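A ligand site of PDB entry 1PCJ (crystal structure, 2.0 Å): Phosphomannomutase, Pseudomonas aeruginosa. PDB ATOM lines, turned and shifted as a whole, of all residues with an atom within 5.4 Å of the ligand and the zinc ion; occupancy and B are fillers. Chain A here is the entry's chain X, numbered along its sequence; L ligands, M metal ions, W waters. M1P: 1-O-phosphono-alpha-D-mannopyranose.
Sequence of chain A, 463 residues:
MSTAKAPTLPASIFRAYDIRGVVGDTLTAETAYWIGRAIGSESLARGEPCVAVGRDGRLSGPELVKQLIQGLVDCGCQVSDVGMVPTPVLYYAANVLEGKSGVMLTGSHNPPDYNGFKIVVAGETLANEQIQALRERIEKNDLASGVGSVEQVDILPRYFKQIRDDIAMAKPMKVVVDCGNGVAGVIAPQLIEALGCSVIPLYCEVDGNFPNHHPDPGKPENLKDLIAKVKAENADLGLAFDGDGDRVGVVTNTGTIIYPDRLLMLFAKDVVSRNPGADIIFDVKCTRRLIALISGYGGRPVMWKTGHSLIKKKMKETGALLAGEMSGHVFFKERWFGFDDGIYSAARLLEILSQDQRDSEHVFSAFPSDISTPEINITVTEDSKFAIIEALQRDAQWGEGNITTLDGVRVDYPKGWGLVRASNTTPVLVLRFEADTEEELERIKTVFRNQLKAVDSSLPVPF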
ATOM      1  N   TYR A  17      26.779   0.092  -4.589  1.00  0.00           N
ATOM      2  CA  TYR A  17      26.487   1.193  -5.527  1.00  0.00           C
ATOM      3  C   TYR A  17      27.261   2.475  -5.192  1.00  0.00           C
ATOM      4  O   TYR A  17      27.502   3.320  -6.062  1.00  0.00           O
ATOM      5  CB  TYR A  17      24.997   1.579  -5.485  1.00  0.00           C
ATOM      6  CG  TYR A  17      23.989   0.458  -5.606  1.00  0.00           C
ATOM      7  CD1 TYR A  17      24.269  -0.704  -6.339  1.00  0.00           C
ATOM      8  CD2 TYR A  17      22.760   0.545  -4.983  1.00  0.00           C
ATOM      9  CE1 TYR A  17      23.360  -1.722  -6.449  1.00  0.00           C
ATOM     10  CE2 TYR A  17      21.808  -0.471  -5.107  1.00  0.00           C
ATOM     11  CZ  TYR A  17      22.123  -1.611  -5.827  1.00  0.00           C
ATOM     12  OH  TYR A  17      21.200  -2.620  -5.922  1.00  0.00           O
ATOM     13  N   ARG A  20      27.360   4.719   1.997  1.00  0.00           N
ATOM     14  CA  ARG A  20      26.138   5.147   2.713  1.00  0.00           C
ATOM     15  C   ARG A  20      26.355   4.894   4.208  1.00  0.00           C
ATOM     16  O   ARG A  20      26.745   3.784   4.606  1.00  0.00           O
ATOM     17  CB  ARG A  20      24.899   4.355   2.240  1.00  0.00           C
ATOM     18  CG  ARG A  20      24.347   4.714   0.833  1.00  0.00           C
ATOM     19  CD  ARG A  20      23.195   3.792   0.307  1.00  0.00           C
ATOM     20  NE  ARG A  20      23.064   3.913  -1.159  1.00  0.00           N
ATOM     21  CZ  ARG A  20      22.025   4.478  -1.825  1.00  0.00           C
ATOM     22  NH1 ARG A  20      20.949   4.932  -1.199  1.00  0.00           N
ATOM     23  NH2 ARG A  20      22.072   4.547  -3.163  1.00  0.00           N
ATOM     24  N   SEP A 108      20.619  10.530  -0.089  1.00  0.00           N
ATOM     25  CA  SEP A 108      19.520  10.178  -0.991  1.00  0.00           C
ATOM     26  CB  SEP A 108      19.698   8.741  -1.519  1.00  0.00           C
ATOM     27  OG  SEP A 108      18.679   8.448  -2.470  1.00  0.00           O
ATOM     28  C   SEP A 108      18.126  10.441  -0.383  1.00  0.00           C
ATOM     29  O   SEP A 108      17.781  11.587  -0.121  1.00  0.00           O
ATOM     30  P   SEP A 108      18.973   7.279  -3.554  1.00  0.00           P
ATOM     31  O1P SEP A 108      18.239   5.977  -3.011  1.00  0.00           O
ATOM     32  O2P SEP A 108      20.558   7.008  -3.702  1.00  0.00           O
ATOM     33  O3P SEP A 108      18.351   7.723  -4.945  1.00  0.00           O
ATOM     34  N   HIS A 109      17.348   9.380  -0.138  1.00  0.00           N
ATOM     35  CA  HIS A 109      15.960   9.495   0.348  1.00  0.00           C
ATOM     36  C   HIS A 109      15.841   9.140   1.833  1.00  0.00           C
ATOM     37  O   HIS A 109      14.743   9.147   2.398  1.00  0.00           O
ATOM     38  CB  HIS A 109      15.067   8.546  -0.457  1.00  0.00           C
ATOM     39  CG  HIS A 109      15.326   7.090  -0.176  1.00  0.00           C
ATOM     40  ND1 HIS A 109      16.316   6.365  -0.806  1.00  0.00           N
ATOM     41  CD2 HIS A 109      14.718   6.229   0.688  1.00  0.00           C
ATOM     42  CE1 HIS A 109      16.315   5.119  -0.346  1.00  0.00           C
ATOM     43  NE2 HIS A 109      15.354   5.009   0.552  1.00  0.00           N
ATOM     44  N   LYS A 118      28.295   9.396  -3.641  1.00  0.00           N
ATOM     45  CA  LYS A 118      28.190   8.802  -4.963  1.00  0.00           C
ATOM     46  C   LYS A 118      29.358   9.337  -5.771  1.00  0.00           C
ATOM     47  O   LYS A 118      29.615  10.563  -5.782  1.00  0.00           O
ATOM     48  CB  LYS A 118      26.835   9.139  -5.588  1.00  0.00           C
ATOM     49  CG  LYS A 118      25.678   8.743  -4.690  1.00  0.00           C
ATOM     50  CD  LYS A 118      24.340   9.154  -5.260  1.00  0.00           C
ATOM     51  CE  LYS A 118      23.221   8.412  -4.611  1.00  0.00           C
ATOM     52  NZ  LYS A 118      21.912   8.853  -5.146  1.00  0.00           N
ATOM     53  N   ASP A 242      12.745  12.778  -5.035  1.00  0.00           N
ATOM     54  CA  ASP A 242      13.364  12.255  -3.838  1.00  0.00           C
ATOM     55  C   ASP A 242      14.355  13.287  -3.301  1.00  0.00           C
ATOM     56  O   ASP A 242      14.526  14.361  -3.904  1.00  0.00           O
ATOM     57  CB  ASP A 242      13.975  10.856  -4.071  1.00  0.00           C
ATOM     58  CG  ASP A 242      15.379  10.871  -4.685  1.00  0.00           C
ATOM     59  OD1 ASP A 242      15.704  11.798  -5.463  1.00  0.00           O
ATOM     60  OD2 ASP A 242      16.219   9.961  -4.460  1.00  0.00           O
ATOM     61  N   GLY A 243      14.986  12.987  -2.180  1.00  0.00           N
ATOM     62  CA  GLY A 243      15.810  13.967  -1.469  1.00  0.00           C
ATOM     63  C   GLY A 243      16.908  14.624  -2.298  1.00  0.00           C
ATOM     64  O   GLY A 243      17.162  15.810  -2.133  1.00  0.00           O
ATOM     65  N   ASP A 244      17.551  13.873  -3.176  1.00  0.00           N
ATOM     66  CA  ASP A 244      18.696  14.396  -3.924  1.00  0.00           C
ATOM     67  C   ASP A 244      18.403  14.642  -5.404  1.00  0.00           C
ATOM     68  O   ASP A 244      19.273  15.068  -6.163  1.00  0.00           O
ATOM     69  CB  ASP A 244      19.938  13.517  -3.711  1.00  0.00           C
ATOM     70  CG  ASP A 244      19.742  12.079  -4.193  1.00  0.00           C
ATOM     71  OD1 ASP A 244      20.701  11.448  -4.676  1.00  0.00           O
ATOM     72  OD2 ASP A 244      18.656  11.491  -4.085  1.00  0.00           O
ATOM     73  N   GLY A 245      17.161  14.389  -5.816  1.00  0.00           N
ATOM     74  CA  GLY A 245      16.680  14.739  -7.139  1.00  0.00           C
ATOM     75  C   GLY A 245      17.020  13.801  -8.285  1.00  0.00           C
ATOM     76  O   GLY A 245      16.789  14.177  -9.448  1.00  0.00           O
ATOM     77  N   ASP A 246      17.576  12.627  -8.002  1.00  0.00           N
ATOM     78  CA  ASP A 246      17.847  11.664  -9.061  1.00  0.00           C
ATOM     79  C   ASP A 246      16.720  10.655  -9.282  1.00  0.00           C
ATOM     80  O   ASP A 246      16.831   9.789 -10.156  1.00  0.00           O
ATOM     81  CB  ASP A 246      19.185  10.939  -8.836  1.00  0.00           C
ATOM     82  CG  ASP A 246      19.251  10.202  -7.538  1.00  0.00           C
ATOM     83  OD1 ASP A 246      18.285  10.190  -6.753  1.00  0.00           O
ATOM     84  OD2 ASP A 246      20.287   9.603  -7.196  1.00  0.00           O
ATOM     85  N   ARG A 247      15.658  10.755  -8.481  1.00  0.00           N
ATOM     86  CA  ARG A 247      14.451   9.971  -8.690  1.00  0.00           C
ATOM     87  C   ARG A 247      13.254  10.896  -8.824  1.00  0.00           C
ATOM     88  O   ARG A 247      13.193  11.940  -8.183  1.00  0.00           O
ATOM     89  CB  ARG A 247      14.195   9.047  -7.516  1.00  0.00           C
ATOM     90  CG  ARG A 247      15.242   7.983  -7.339  1.00  0.00           C
ATOM     91  CD  ARG A 247      14.749   6.808  -6.580  1.00  0.00           C
ATOM     92  NE  ARG A 247      14.618   7.114  -5.167  1.00  0.00           N
ATOM     93  CZ  ARG A 247      13.736   6.537  -4.345  1.00  0.00           C
ATOM     94  NH1 ARG A 247      12.877   5.613  -4.774  1.00  0.00           N
ATOM     95  NH2 ARG A 247      13.718   6.905  -3.081  1.00  0.00           N
ATOM     96  N   ASP A 283      15.637  -2.331 -15.193  1.00  0.00           N
ATOM     97  CA  ASP A 283      16.031  -3.316 -14.201  1.00  0.00           C
ATOM     98  C   ASP A 283      15.036  -4.463 -14.020  1.00  0.00           C
ATOM     99  O   ASP A 283      13.889  -4.394 -14.480  1.00  0.00           O
ATOM    100  CB  ASP A 283      16.416  -2.661 -12.867  1.00  0.00           C
ATOM    101  CG  ASP A 283      15.247  -2.201 -12.082  1.00  0.00           C
ATOM    102  OD1 ASP A 283      15.208  -2.434 -10.842  1.00  0.00           O
ATOM    103  OD2 ASP A 283      14.326  -1.568 -12.609  1.00  0.00           O
ATOM    104  N   LYS A 285      13.262  -5.338 -11.750  1.00  0.00           N
ATOM    105  CA  LYS A 285      12.015  -5.013 -11.032  1.00  0.00           C
ATOM    106  C   LYS A 285      10.888  -4.452 -11.909  1.00  0.00           C
ATOM    107  O   LYS A 285       9.778  -4.212 -11.394  1.00  0.00           O
ATOM    108  CB  LYS A 285      12.307  -4.031  -9.888  1.00  0.00           C
ATOM    109  CG  LYS A 285      13.064  -4.644  -8.729  1.00  0.00           C
ATOM    110  CD  LYS A 285      13.589  -3.595  -7.736  1.00  0.00           C
ATOM    111  CE  LYS A 285      12.495  -2.964  -6.902  1.00  0.00           C
ATOM    112  NZ  LYS A 285      12.843  -1.560  -6.473  1.00  0.00           N
ATOM    113  N   THR A 306      19.317  -4.237 -10.875  1.00  0.00           N
ATOM    114  CA  THR A 306      18.919  -3.098 -10.076  1.00  0.00           C
ATOM    115  C   THR A 306      20.142  -2.378  -9.505  1.00  0.00           C
ATOM    116  O   THR A 306      21.138  -3.005  -9.147  1.00  0.00           O
ATOM    117  CB  THR A 306      18.056  -3.631  -8.915  1.00  0.00           C
ATOM    118  OG1 THR A 306      16.843  -4.210  -9.438  1.00  0.00           O
ATOM    119  CG2 THR A 306      17.616  -2.509  -7.983  1.00  0.00           C
ATOM    120  N   GLY A 307      20.041  -1.044  -9.391  1.00  0.00           N
ATOM    121  CA  GLY A 307      21.075  -0.224  -8.775  1.00  0.00           C
ATOM    122  C   GLY A 307      21.595   0.794  -9.745  1.00  0.00           C
ATOM    123  O   GLY A 307      22.108   0.418 -10.797  1.00  0.00           O
ATOM    124  N   HIS A 308      21.525   2.078  -9.378  1.00  0.00           N
ATOM    125  CA  HIS A 308      21.844   3.168 -10.270  1.00  0.00           C
ATOM    126  C   HIS A 308      23.234   3.065 -10.909  1.00  0.00           C
ATOM    127  O   HIS A 308      23.367   3.228 -12.113  1.00  0.00           O
ATOM    128  CB  HIS A 308      21.675   4.526  -9.558  1.00  0.00           C
ATOM    129  CG  HIS A 308      22.738   4.809  -8.539  1.00  0.00           C
ATOM    130  ND1 HIS A 308      23.701   5.789  -8.725  1.00  0.00           N
ATOM    131  CD2 HIS A 308      23.009   4.237  -7.344  1.00  0.00           C
ATOM    132  CE1 HIS A 308      24.492   5.828  -7.669  1.00  0.00           C
ATOM    133  NE2 HIS A 308      24.101   4.897  -6.815  1.00  0.00           N
ATOM    134  N   GLU A 325      14.904   2.532 -13.927  1.00  0.00           N
ATOM    135  CA  GLU A 325      14.642   1.577 -12.866  1.00  0.00           C
ATOM    136  C   GLU A 325      13.255   1.762 -12.310  1.00  0.00           C
ATOM    137  O   GLU A 325      12.700   2.863 -12.345  1.00  0.00           O
ATOM    138  CB  GLU A 325      15.572   1.795 -11.708  1.00  0.00           C
ATOM    139  CG  GLU A 325      17.023   1.584 -12.023  1.00  0.00           C
ATOM    140  CD  GLU A 325      17.802   1.539 -10.751  1.00  0.00           C
ATOM    141  OE1 GLU A 325      17.879   0.426 -10.183  1.00  0.00           O
ATOM    142  OE2 GLU A 325      18.266   2.617 -10.292  1.00  0.00           O
ATOM    143  N   SER A 327      12.546   2.029  -9.343  1.00  0.00           N
ATOM    144  CA  SER A 327      12.645   3.007  -8.254  1.00  0.00           C
ATOM    145  C   SER A 327      12.515   4.458  -8.728  1.00  0.00           C
ATOM    146  O   SER A 327      12.379   5.367  -7.919  1.00  0.00           O
ATOM    147  CB  SER A 327      13.972   2.837  -7.511  1.00  0.00           C
ATOM    148  OG  SER A 327      15.073   3.013  -8.389  1.00  0.00           O
ATOM    149  N   HIS A 329      14.826   6.042 -10.923  1.00  0.00           N
ATOM    150  CA  HIS A 329      16.064   6.529 -11.529  1.00  0.00           C
ATOM    151  C   HIS A 329      15.895   6.341 -13.024  1.00  0.00           C
ATOM    152  O   HIS A 329      15.751   5.216 -13.475  1.00  0.00           O
ATOM    153  CB  HIS A 329      17.298   5.702 -11.089  1.00  0.00           C
ATOM    154  CG  HIS A 329      17.716   5.916  -9.670  1.00  0.00           C
ATOM    155  ND1 HIS A 329      18.241   7.105  -9.218  1.00  0.00           N
ATOM    156  CD2 HIS A 329      17.725   5.082  -8.617  1.00  0.00           C
ATOM    157  CE1 HIS A 329      18.507   7.000  -7.932  1.00  0.00           C
ATOM    158  NE2 HIS A 329      18.211   5.784  -7.535  1.00  0.00           N
ATOM    159  N   ARG A 421      15.384 -11.083  -5.245  1.00  0.00           N
ATOM    160  CA  ARG A 421      16.782 -10.667  -5.239  1.00  0.00           C
ATOM    161  C   ARG A 421      17.177 -10.072  -3.885  1.00  0.00           C
ATOM    162  O   ARG A 421      16.318  -9.672  -3.099  1.00  0.00           O
ATOM    163  CB  ARG A 421      17.036  -9.631  -6.330  1.00  0.00           C
ATOM    164  CG  ARG A 421      16.195  -8.385  -6.204  1.00  0.00           C
ATOM    165  CD  ARG A 421      16.519  -7.329  -7.218  1.00  0.00           C
ATOM    166  NE  ARG A 421      17.767  -6.612  -6.937  1.00  0.00           N
ATOM    167  CZ  ARG A 421      17.917  -5.675  -6.003  1.00  0.00           C
ATOM    168  NH1 ARG A 421      16.917  -5.327  -5.220  1.00  0.00           N
ATOM    169  NH2 ARG A 421      19.087  -5.068  -5.865  1.00  0.00           N
ATOM    170  N   ALA A 422      18.483  -9.999  -3.642  1.00  0.00           N
ATOM    171  CA  ALA A 422      19.034  -9.334  -2.476  1.00  0.00           C
ATOM    172  C   ALA A 422      19.174  -7.841  -2.723  1.00  0.00           C
ATOM    173  O   ALA A 422      19.752  -7.409  -3.720  1.00  0.00           O
ATOM    174  CB  ALA A 422      20.396  -9.923  -2.148  1.00  0.00           C
ATOM    175  N   SER A 423      18.667  -7.052  -1.784  1.00  0.00           N
ATOM    176  CA  SER A 423      18.932  -5.627  -1.759  1.00  0.00           C
ATOM    177  C   SER A 423      20.423  -5.389  -1.475  1.00  0.00           C
ATOM    178  O   SER A 423      21.062  -6.154  -0.737  1.00  0.00           O
ATOM    179  CB  SER A 423      18.064  -4.954  -0.671  1.00  0.00           C
ATOM    180  OG  SER A 423      18.575  -3.688  -0.286  1.00  0.00           O
ATOM    181  N   ASN A 424      20.970  -4.344  -2.076  1.00  0.00           N
ATOM    182  CA  ASN A 424      22.347  -3.932  -1.827  1.00  0.00           C
ATOM    183  C   ASN A 424      22.440  -2.666  -0.964  1.00  0.00           C
ATOM    184  O   ASN A 424      23.512  -2.060  -0.874  1.00  0.00           O
ATOM    185  CB  ASN A 424      23.083  -3.708  -3.157  1.00  0.00           C
ATOM    186  CG  ASN A 424      23.213  -4.969  -3.965  1.00  0.00           C
ATOM    187  OD1 ASN A 424      22.623  -5.102  -5.065  1.00  0.00           O
ATOM    188  ND2 ASN A 424      23.976  -5.924  -3.455  1.00  0.00           N
ATOM    189  N   THR A 425      21.315  -2.260  -0.359  1.00  0.00           N
ATOM    190  CA  THR A 425      21.288  -1.108   0.552  1.00  0.00           C
ATOM    191  C   THR A 425      20.767  -1.440   1.948  1.00  0.00           C
ATOM    192  O   THR A 425      20.926  -0.628   2.861  1.00  0.00           O
ATOM    193  CB  THR A 425      20.418   0.049  -0.009  1.00  0.00           C
ATOM    194  OG1 THR A 425      19.045  -0.361  -0.122  1.00  0.00           O
ATOM    195  CG2 THR A 425      20.828   0.446  -1.425  1.00  0.00           C
ATOM    196  N   THR A 426      20.127  -2.604   2.097  1.00  0.00           N
ATOM    197  CA  THR A 426      19.491  -3.047   3.341  1.00  0.00           C
ATOM    198  C   THR A 426      19.582  -4.580   3.444  1.00  0.00           C
ATOM    199  O   THR A 426      19.785  -5.222   2.434  1.00  0.00           O
ATOM    200  CB  THR A 426      17.986  -2.636   3.375  1.00  0.00           C
ATOM    201  OG1 THR A 426      17.280  -3.266   2.279  1.00  0.00           O
ATOM    202  CG2 THR A 426      17.806  -1.140   3.167  1.00  0.00           C
ATOM    203  N   VAL A 430      14.145  -8.699  -1.745  1.00  0.00           N
ATOM    204  CA  VAL A 430      13.151  -7.896  -2.445  1.00  0.00           C
ATOM    205  C   VAL A 430      12.420  -8.820  -3.426  1.00  0.00           C
ATOM    206  O   VAL A 430      13.051  -9.529  -4.201  1.00  0.00           O
ATOM    207  CB  VAL A 430      13.823  -6.761  -3.229  1.00  0.00           C
ATOM    208  CG1 VAL A 430      12.789  -5.899  -3.948  1.00  0.00           C
ATOM    209  CG2 VAL A 430      14.704  -5.915  -2.295  1.00  0.00           C
HETATM  210  O6  M1P L   1      18.491   4.407  -5.058  1.00  0.00           O
HETATM  211  C6  M1P L   1      19.511   3.416  -4.951  1.00  0.00           C
HETATM  212  C5  M1P L   1      18.905   2.050  -5.253  1.00  0.00           C
HETATM  213  O5  M1P L   1      18.036   1.642  -4.129  1.00  0.00           O
HETATM  214  C1  M1P L   1      17.459   0.311  -4.326  1.00  0.00           C
HETATM  215  O1  M1P L   1      18.486  -0.646  -4.442  1.00  0.00           O
HETATM  216  P   M1P L   1      18.287  -2.050  -3.690  1.00  0.00           P
HETATM  217  O1P M1P L   1      17.082  -2.775  -4.222  1.00  0.00           O
HETATM  218  O2P M1P L   1      18.124  -1.820  -2.206  1.00  0.00           O
HETATM  219  O3P M1P L   1      19.523  -2.855  -3.984  1.00  0.00           O
HETATM  220  C2  M1P L   1      16.647   0.262  -5.616  1.00  0.00           C
HETATM  221  O2  M1P L   1      15.497   1.147  -5.441  1.00  0.00           O
HETATM  222  C3  M1P L   1      17.495   0.735  -6.832  1.00  0.00           C
HETATM  223  O3  M1P L   1      16.656   0.838  -7.980  1.00  0.00           O
HETATM  224  C4  M1P L   1      18.131   2.095  -6.559  1.00  0.00           C
HETATM  225  O4  M1P L   1      19.033   2.437  -7.617  1.00  0.00           O
HETATM  226 ZN    ZN M   1      18.067   9.787  -4.935  1.00  0.00          ZN
HETATM  227  O   HOH W   1      13.814   0.322  -3.706  1.00  0.00           O
HETATM  228  O   HOH W   2      15.653  -1.345  -1.288  1.00  0.00           O
HETATM  229  O   HOH W   3      14.502  -2.576  -4.193  1.00  0.00           O
HETATM  230  O   HOH W   4      14.458  -0.393  -9.046  1.00  0.00           O
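The side-chain hydroxyl of Ser 327 lies within hydrogen-bond range of an oxygen (O3) of the ligand, at 2.7 Å. O3P of the ligand lies within hydrogen-bond range of OH of Tyr 17 (2.6 Å). The side-chain hydroxyl (OG1) of Thr 425 is in hydrogen-bond range of an oxygen (O2P) of the ligand, at 2.7 Å. NE2 of His 329 sits at hydrogen-bond distance from O6 of the ligand, at 2.8 Å. An oxygen (O2P) of the ligand lies within hydrogen-bond range of the side-chain hydroxyl of Ser 423. O1P of the ligand is in salt-bridge range of NH1 of Arg 421 (2.7 Å). O1P of SEP 108 is in hydrogen-bond range of an oxygen (O6) of the ligand (2.6 Å). O4 of the ligand is in hydrogen-bond range of N of His 308, at 3.1 Å. N of Asn 424 sits at hydrogen-bond distance from O3P of the ligand (2.8 Å). An oxygen (O3) of the ligand lies within hydrogen-bond range of the side-chain carboxylate (OE1) of Glu 325, at 2.6 Å.
The side-chain hydroxyl of Thr 426 lies within hydrogen-bond range of the side-chain hydroxyl of Ser 423. OE2 of Glu 325 lies within hydrogen-bond range of N of His 308 (3.4 Å). O of Asp 246 lies within hydrogen-bond range of ND1 of His 329, at 3.2 Å. OG1 of Thr 306 is in hydrogen-bond range of OD1 of Asp 283 (2.8 Å). O2P of SEP 108 is in salt-bridge range of NZ of Lys 118, 2.7 Å away. O2P of SEP 108 lies within salt-bridge range of NH2 of Arg 20, 2.9 Å away. O of Arg 421 lies within hydrogen-bond range of N of Val 430, at 2.7 Å. OD2 of Asp 246 lies within salt-bridge range of NZ of Lys 118 (2.7 Å).
Residues that only touch the ligand: Arg 20 (3.3 Å), Lys 285 (3.9 Å), Thr 306 (3.4 Å) and Gly 307 (3.5 Å). Hydrophobic or aromatic side chains within 4 Å of the ligand: Tyr 17, His 308 and His 329.
Lys 118 touches the zinc ion (NZ to ZN, 3.96 Å). Within 4 Å of the zinc ion: SEP 108, Lys 118, Asp 242, Asp 244 and Asp 246. Along chain A the residues within 4 Å of the zinc ion span positions 108 to 246. The nearest printed residue that does not touch the zinc ion is His 329 (4.1 Å).
The zinc ion is bound by OD1 of Asp 246 (1.9 Å). The side-chain carboxylate (OD2) of Asp 242 is bound to the zinc ion, 1.9 Å away. The side-chain carboxylate (OD2) of Asp 244 binds the zinc ion (2.0 Å). O3P of SEP 108 binds the zinc ion, at 2.1 Å. The zinc ion has four donor atoms within binding distance.
Water W1 bridges an oxygen (O2) of the ligand (2.6 Å) and the side-chain amino group (NZ) of Lys 285 (3.5 Å). Water W3 bridges an oxygen (O1P) of the ligand (2.6 Å) and the side-chain amino group of Lys 285 (3.0 Å). Water W4 lies within hydrogen-bond range of O3 of the ligand, OD1 of Asp 283, N of Ser 327 and NZ of Lys 285.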
